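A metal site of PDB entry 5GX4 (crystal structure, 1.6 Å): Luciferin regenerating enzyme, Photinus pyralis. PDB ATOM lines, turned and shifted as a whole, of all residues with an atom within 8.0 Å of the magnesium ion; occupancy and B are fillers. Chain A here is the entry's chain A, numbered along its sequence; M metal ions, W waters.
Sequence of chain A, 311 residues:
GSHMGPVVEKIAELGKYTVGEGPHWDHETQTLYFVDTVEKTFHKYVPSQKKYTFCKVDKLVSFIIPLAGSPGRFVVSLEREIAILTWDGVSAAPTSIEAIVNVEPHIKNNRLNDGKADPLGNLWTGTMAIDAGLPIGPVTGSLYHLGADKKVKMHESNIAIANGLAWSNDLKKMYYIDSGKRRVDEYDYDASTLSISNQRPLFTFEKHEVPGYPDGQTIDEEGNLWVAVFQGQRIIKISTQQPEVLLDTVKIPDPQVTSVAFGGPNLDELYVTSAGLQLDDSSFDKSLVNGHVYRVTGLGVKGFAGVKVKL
Of the 27 residues printed, 3 come within 4 Å of the magnesium ion.
The magnesium ion is bound by the side-chain carboxylate of Glu 21 (2.0 Å), the side-chain amide oxygen of Asn 163 (2.0 Å), water W3 (2.0 Å), water W1 (2.1 Å), the side-chain carboxylate of Asp 215 (2.1 Å) and water W2 (2.2 Å).
ND2 of Asn 163 lies within hydrogen-bond range of OG of Ser 179, 2.7 Å away.
N of Asn 163 sits at hydrogen-bond distance from O of Ile 177.
The backbone NH of Gly 164 sits at hydrogen-bond distance from the backbone carbonyl oxygen of Asp 215, at 3.0 Å.
N of Asp 215 is in hydrogen-bond range of O of Ala 228 (3.0 Å).
Water W2 lies within hydrogen-bond range of the side-chain amide oxygen (OD1) of Asn 113 (3.0 Å) and the side-chain carboxylate (OE2) of Glu 21 (3.3 Å).
Water W1 lies within hydrogen-bond range of ND2 of Asn 113 (3.1 Å) and ND2 of Asn 163 (3.2 Å).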
ATOM      1  N   VAL A  19       6.160  28.714  15.394  1.00  0.00           N
ATOM      2  CA  VAL A  19       6.989  28.566  16.589  1.00  0.00           C
ATOM      3  C   VAL A  19       8.449  28.570  16.143  1.00  0.00           C
ATOM      4  O   VAL A  19       9.042  27.498  15.937  1.00  0.00           O
ATOM      5  CB  VAL A  19       6.653  27.293  17.387  1.00  0.00           C
ATOM      6  CG1 VAL A  19       7.469  27.251  18.688  1.00  0.00           C
ATOM      7  CG2 VAL A  19       5.156  27.188  17.712  1.00  0.00           C
ATOM      8  N   GLY A  20       9.033  29.749  15.936  1.00  0.00           N
ATOM      9  CA  GLY A  20      10.461  29.824  15.670  1.00  0.00           C
ATOM     10  C   GLY A  20      11.238  29.368  16.897  1.00  0.00           C
ATOM     11  O   GLY A  20      10.860  29.670  18.027  1.00  0.00           O
ATOM     12  N   GLU A  21      12.327  28.649  16.668  1.00  0.00           N
ATOM     13  CA  GLU A  21      12.999  27.890  17.729  1.00  0.00           C
ATOM     14  C   GLU A  21      14.397  27.487  17.300  1.00  0.00           C
ATOM     15  O   GLU A  21      14.782  27.595  16.127  1.00  0.00           O
ATOM     16  CB  GLU A  21      12.196  26.631  18.115  1.00  0.00           C
ATOM     17  CG  GLU A  21      11.303  26.786  19.320  1.00  0.00           C
ATOM     18  CD  GLU A  21      12.067  26.674  20.605  1.00  0.00           C
ATOM     19  OE1 GLU A  21      11.446  26.488  21.676  1.00  0.00           O
ATOM     20  OE2 GLU A  21      13.316  26.778  20.564  1.00  0.00           O
ATOM     21  N   GLY A  22      15.166  26.965  18.273  1.00  0.00           N
ATOM     22  CA  GLY A  22      16.452  26.336  18.020  1.00  0.00           C
ATOM     23  C   GLY A  22      17.488  27.170  17.270  1.00  0.00           C
ATOM     24  O   GLY A  22      18.147  26.651  16.366  1.00  0.00           O
ATOM     25  N   PRO A  23      17.696  28.436  17.641  1.00  0.00           N
ATOM     26  CA  PRO A  23      18.706  29.232  16.938  1.00  0.00           C
ATOM     27  C   PRO A  23      20.116  28.707  17.191  1.00  0.00           C
ATOM     28  O   PRO A  23      20.462  28.312  18.316  1.00  0.00           O
ATOM     29  CB  PRO A  23      18.527  30.639  17.510  1.00  0.00           C
ATOM     30  CG  PRO A  23      18.021  30.389  18.903  1.00  0.00           C
ATOM     31  CD  PRO A  23      17.107  29.185  18.764  1.00  0.00           C
ATOM     32  N   THR A  37       9.103  24.619  14.952  1.00  0.00           N
ATOM     33  CA  THR A  37       8.829  23.302  15.524  1.00  0.00           C
ATOM     34  C   THR A  37       7.449  22.784  15.181  1.00  0.00           C
ATOM     35  O   THR A  37       7.161  21.629  15.489  1.00  0.00           O
ATOM     36  CB  THR A  37       8.989  23.297  17.056  1.00  0.00           C
ATOM     37  OG1 THR A  37       8.165  24.316  17.642  1.00  0.00           O
ATOM     38  CG2 THR A  37      10.430  23.513  17.444  1.00  0.00           C
ATOM     39  N   SER A  62      13.018  20.036  15.519  1.00  0.00           N
ATOM     40  CA  SER A  62      13.229  20.879  16.696  1.00  0.00           C
ATOM     41  C   SER A  62      14.632  21.450  16.874  1.00  0.00           C
ATOM     42  O   SER A  62      14.801  22.329  17.730  1.00  0.00           O
ATOM     43  CB  SER A  62      12.844  20.094  17.958  1.00  0.00           C
ATOM     44  OG  SER A  62      13.662  18.954  18.157  1.00  0.00           O
ATOM     45  N   ASN A 113      12.498  17.570  21.229  1.00  0.00           N
ATOM     46  CA  ASN A 113      12.364  19.022  21.334  1.00  0.00           C
ATOM     47  C   ASN A 113      13.764  19.627  21.381  1.00  0.00           C
ATOM     48  O   ASN A 113      14.559  19.361  20.481  1.00  0.00           O
ATOM     49  CB  ASN A 113      11.460  19.412  22.486  1.00  0.00           C
ATOM     50  CG  ASN A 113      10.993  20.855  22.372  1.00  0.00           C
ATOM     51  OD1 ASN A 113      10.874  21.395  21.258  1.00  0.00           O
ATOM     52  ND2 ASN A 113      10.696  21.486  23.502  1.00  0.00           N
ATOM     53  N   ASP A 114      14.094  20.437  22.376  1.00  0.00           N
ATOM     54  CA  ASP A 114      15.324  21.223  22.260  1.00  0.00           C
ATOM     55  C   ASP A 114      16.562  20.320  22.286  1.00  0.00           C
ATOM     56  O   ASP A 114      16.582  19.288  22.953  1.00  0.00           O
ATOM     57  CB  ASP A 114      15.388  22.290  23.367  1.00  0.00           C
ATOM     58  CG  ASP A 114      16.085  23.576  22.895  1.00  0.00           C
ATOM     59  OD1 ASP A 114      16.609  23.623  21.750  1.00  0.00           O
ATOM     60  OD2 ASP A 114      16.122  24.577  23.669  1.00  0.00           O
ATOM     61  N   GLY A 115      17.566  20.702  21.508  1.00  0.00           N
ATOM     62  CA  GLY A 115      18.826  19.970  21.459  1.00  0.00           C
ATOM     63  C   GLY A 115      19.963  20.943  21.240  1.00  0.00           C
ATOM     64  O   GLY A 115      19.802  22.007  20.636  1.00  0.00           O
ATOM     65  N   MET A 128       9.345  14.854  24.534  1.00  0.00           N
ATOM     66  CA  MET A 128       8.100  15.313  25.150  1.00  0.00           C
ATOM     67  C   MET A 128       6.943  14.717  24.363  1.00  0.00           C
ATOM     68  O   MET A 128       7.106  14.295  23.214  1.00  0.00           O
ATOM     69  CB  MET A 128       7.999  16.843  25.137  1.00  0.00           C
ATOM     70  CG  MET A 128       7.972  17.387  23.705  1.00  0.00           C
ATOM     71  SD  MET A 128       7.932  19.192  23.568  1.00  0.00           S
ATOM     72  CE  MET A 128       6.180  19.505  23.776  1.00  0.00           C
ATOM     73  N   ILE A 161       8.117  19.227  29.197  1.00  0.00           N
ATOM     74  CA  ILE A 161       8.487  19.904  27.956  1.00  0.00           C
ATOM     75  C   ILE A 161      10.002  20.104  27.993  1.00  0.00           C
ATOM     76  O   ILE A 161      10.496  21.023  28.652  1.00  0.00           O
ATOM     77  CB  ILE A 161       7.730  21.221  27.764  1.00  0.00           C
ATOM     78  CG1 ILE A 161       6.238  20.947  27.581  1.00  0.00           C
ATOM     79  CG2 ILE A 161       8.238  21.962  26.531  1.00  0.00           C
ATOM     80  CD1 ILE A 161       5.404  22.198  27.371  1.00  0.00           C
ATOM     81  N   ALA A 162      10.726  19.238  27.290  1.00  0.00           N
ATOM     82  CA  ALA A 162      12.188  19.273  27.263  1.00  0.00           C
ATOM     83  C   ALA A 162      12.700  20.532  26.569  1.00  0.00           C
ATOM     84  O   ALA A 162      12.431  20.740  25.382  1.00  0.00           O
ATOM     85  CB  ALA A 162      12.708  18.028  26.544  1.00  0.00           C
ATOM     86  N   ASN A 163      13.450  21.365  27.283  1.00  0.00           N
ATOM     87  CA  ASN A 163      13.809  22.643  26.668  1.00  0.00           C
ATOM     88  C   ASN A 163      15.268  23.035  26.887  1.00  0.00           C
ATOM     89  O   ASN A 163      16.138  22.176  26.730  1.00  0.00           O
ATOM     90  CB  ASN A 163      12.825  23.722  27.139  1.00  0.00           C
ATOM     91  CG  ASN A 163      11.922  24.133  26.013  1.00  0.00           C
ATOM     92  OD1 ASN A 163      12.386  24.257  24.887  1.00  0.00           O
ATOM     93  ND2 ASN A 163      10.634  24.300  26.283  1.00  0.00           N
ATOM     94  N   GLY A 164      15.566  24.304  27.175  1.00  0.00           N
ATOM     95  CA  GLY A 164      16.909  24.816  26.936  1.00  0.00           C
ATOM     96  C   GLY A 164      18.005  24.180  27.777  1.00  0.00           C
ATOM     97  O   GLY A 164      17.811  23.763  28.922  1.00  0.00           O
ATOM     98  N   ILE A 177      16.262  23.052  31.458  1.00  0.00           N
ATOM     99  CA  ILE A 177      14.906  23.572  31.644  1.00  0.00           C
ATOM    100  C   ILE A 177      13.896  22.524  31.195  1.00  0.00           C
ATOM    101  O   ILE A 177      13.887  22.131  30.023  1.00  0.00           O
ATOM    102  CB  ILE A 177      14.687  24.872  30.864  1.00  0.00           C
ATOM    103  CG1 ILE A 177      15.529  26.001  31.463  1.00  0.00           C
ATOM    104  CG2 ILE A 177      13.184  25.222  30.847  1.00  0.00           C
ATOM    105  CD1 ILE A 177      15.746  27.166  30.496  1.00  0.00           C
ATOM    106  N   SER A 179      10.059  23.047  30.928  1.00  0.00           N
ATOM    107  CA  SER A 179       9.222  24.238  31.047  1.00  0.00           C
ATOM    108  C   SER A 179       8.120  24.059  32.082  1.00  0.00           C
ATOM    109  O   SER A 179       7.734  25.018  32.757  1.00  0.00           O
ATOM    110  CB  SER A 179       8.630  24.610  29.687  1.00  0.00           C
ATOM    111  OG  SER A 179       9.651  24.937  28.762  1.00  0.00           O
ATOM    112  N   PRO A 214       9.939  29.156  31.454  1.00  0.00           N
ATOM    113  CA  PRO A 214      11.268  29.153  30.828  1.00  0.00           C
ATOM    114  C   PRO A 214      11.247  28.231  29.622  1.00  0.00           C
ATOM    115  O   PRO A 214      10.603  27.192  29.626  1.00  0.00           O
ATOM    116  CB  PRO A 214      12.186  28.641  31.942  1.00  0.00           C
ATOM    117  CG  PRO A 214      11.294  27.741  32.761  1.00  0.00           C
ATOM    118  CD  PRO A 214       9.904  28.375  32.707  1.00  0.00           C
ATOM    119  N   ASP A 215      11.948  28.641  28.556  1.00  0.00           N
ATOM    120  CA  ASP A 215      11.943  27.900  27.297  1.00  0.00           C
ATOM    121  C   ASP A 215      13.398  27.633  26.924  1.00  0.00           C
ATOM    122  O   ASP A 215      14.053  26.819  27.595  1.00  0.00           O
ATOM    123  CB  ASP A 215      11.144  28.671  26.233  1.00  0.00           C
ATOM    124  CG  ASP A 215      10.728  27.804  25.020  1.00  0.00           C
ATOM    125  OD1 ASP A 215      11.403  26.804  24.703  1.00  0.00           O
ATOM    126  OD2 ASP A 215       9.716  28.139  24.346  1.00  0.00           O
ATOM    127  N   GLY A 216      13.947  28.312  25.900  1.00  0.00           N
ATOM    128  CA  GLY A 216      15.365  28.130  25.580  1.00  0.00           C
ATOM    129  C   GLY A 216      16.276  28.939  26.500  1.00  0.00           C
ATOM    130  O   GLY A 216      15.845  29.854  27.197  1.00  0.00           O
ATOM    131  N   GLN A 217      17.562  28.586  26.525  1.00  0.00           N
ATOM    132  CA  GLN A 217      18.523  29.381  27.272  1.00  0.00           C
ATOM    133  C   GLN A 217      19.900  29.288  26.644  1.00  0.00           C
ATOM    134  O   GLN A 217      20.204  28.351  25.886  1.00  0.00           O
ATOM    135  CB  GLN A 217      18.608  28.951  28.742  1.00  0.00           C
ATOM    136  CG  GLN A 217      19.173  27.564  28.954  1.00  0.00           C
ATOM    137  CD  GLN A 217      19.258  27.219  30.433  1.00  0.00           C
ATOM    138  OE1 GLN A 217      19.313  28.115  31.292  1.00  0.00           O
ATOM    139  NE2 GLN A 217      19.224  25.923  30.743  1.00  0.00           N
ATOM    140  N   ALA A 228      14.864  32.562  27.743  1.00  0.00           N
ATOM    141  CA  ALA A 228      13.662  33.005  27.061  1.00  0.00           C
ATOM    142  C   ALA A 228      12.426  32.701  27.904  1.00  0.00           C
ATOM    143  O   ALA A 228      12.297  31.607  28.448  1.00  0.00           O
ATOM    144  CB  ALA A 228      13.541  32.307  25.706  1.00  0.00           C
ATOM    145  N   PHE A 230       8.584  32.211  27.747  1.00  0.00           N
ATOM    146  CA  PHE A 230       7.408  32.006  26.919  1.00  0.00           C
ATOM    147  C   PHE A 230       6.170  32.473  27.680  1.00  0.00           C
ATOM    148  O   PHE A 230       5.933  32.033  28.811  1.00  0.00           O
ATOM    149  CB  PHE A 230       7.308  30.510  26.536  1.00  0.00           C
ATOM    150  CG  PHE A 230       6.230  30.201  25.532  1.00  0.00           C
ATOM    151  CD1 PHE A 230       6.529  30.148  24.177  1.00  0.00           C
ATOM    152  CD2 PHE A 230       4.931  29.953  25.951  1.00  0.00           C
ATOM    153  CE1 PHE A 230       5.529  29.846  23.242  1.00  0.00           C
ATOM    154  CE2 PHE A 230       3.926  29.670  25.015  1.00  0.00           C
ATOM    155  CZ  PHE A 230       4.228  29.618  23.670  1.00  0.00           C
ATOM    156  N   VAL A 257       8.236  34.400  23.711  1.00  0.00           N
ATOM    157  CA  VAL A 257       9.672  34.269  23.451  1.00  0.00           C
ATOM    158  C   VAL A 257      10.079  32.821  23.639  1.00  0.00           C
ATOM    159  O   VAL A 257       9.732  32.205  24.662  1.00  0.00           O
ATOM    160  CB  VAL A 257      10.454  35.195  24.386  1.00  0.00           C
ATOM    161  CG1 VAL A 257      11.932  35.139  24.091  1.00  0.00           C
ATOM    162  CG2 VAL A 257       9.927  36.630  24.282  1.00  0.00           C
ATOM    163  N   THR A 258      10.805  32.248  22.668  1.00  0.00           N
ATOM    164  CA  THR A 258      11.094  30.817  22.669  1.00  0.00           C
ATOM    165  C   THR A 258      12.559  30.477  22.888  1.00  0.00           C
ATOM    166  O   THR A 258      12.844  29.496  23.567  1.00  0.00           O
ATOM    167  CB  THR A 258      10.645  30.156  21.352  1.00  0.00           C
ATOM    168  OG1 THR A 258      11.293  30.809  20.246  1.00  0.00           O
ATOM    169  CG2 THR A 258       9.128  30.241  21.177  1.00  0.00           C
ATOM    170  N   SER A 259      13.517  31.198  22.287  1.00  0.00           N
ATOM    171  CA  SER A 259      14.913  30.825  22.502  1.00  0.00           C
ATOM    172  C   SER A 259      15.828  32.006  22.176  1.00  0.00           C
ATOM    173  O   SER A 259      15.375  33.072  21.741  1.00  0.00           O
ATOM    174  CB  SER A 259      15.297  29.585  21.688  1.00  0.00           C
ATOM    175  OG  SER A 259      16.440  28.940  22.260  1.00  0.00           O
ATOM    176  N   THR A 273      14.234  34.211  19.151  1.00  0.00           N
ATOM    177  CA  THR A 273      13.108  33.689  18.385  1.00  0.00           C
ATOM    178  C   THR A 273      11.835  33.772  19.225  1.00  0.00           C
ATOM    179  O   THR A 273      11.888  33.867  20.458  1.00  0.00           O
ATOM    180  CB  THR A 273      13.342  32.223  17.974  1.00  0.00           C
ATOM    181  OG1 THR A 273      13.674  31.457  19.126  1.00  0.00           O
ATOM    182  CG2 THR A 273      14.481  32.120  16.936  1.00  0.00           C
HETATM  183 MG    MG M   1      11.926  25.369  23.247  1.00  0.00          MG
HETATM  184  O   HOH W   1      10.063  24.478  23.096  1.00  0.00           O
HETATM  185  O   HOH W   2      12.606  23.819  21.883  1.00  0.00           O
HETATM  186  O   HOH W   3      13.775  26.223  23.152  1.00  0.00           O
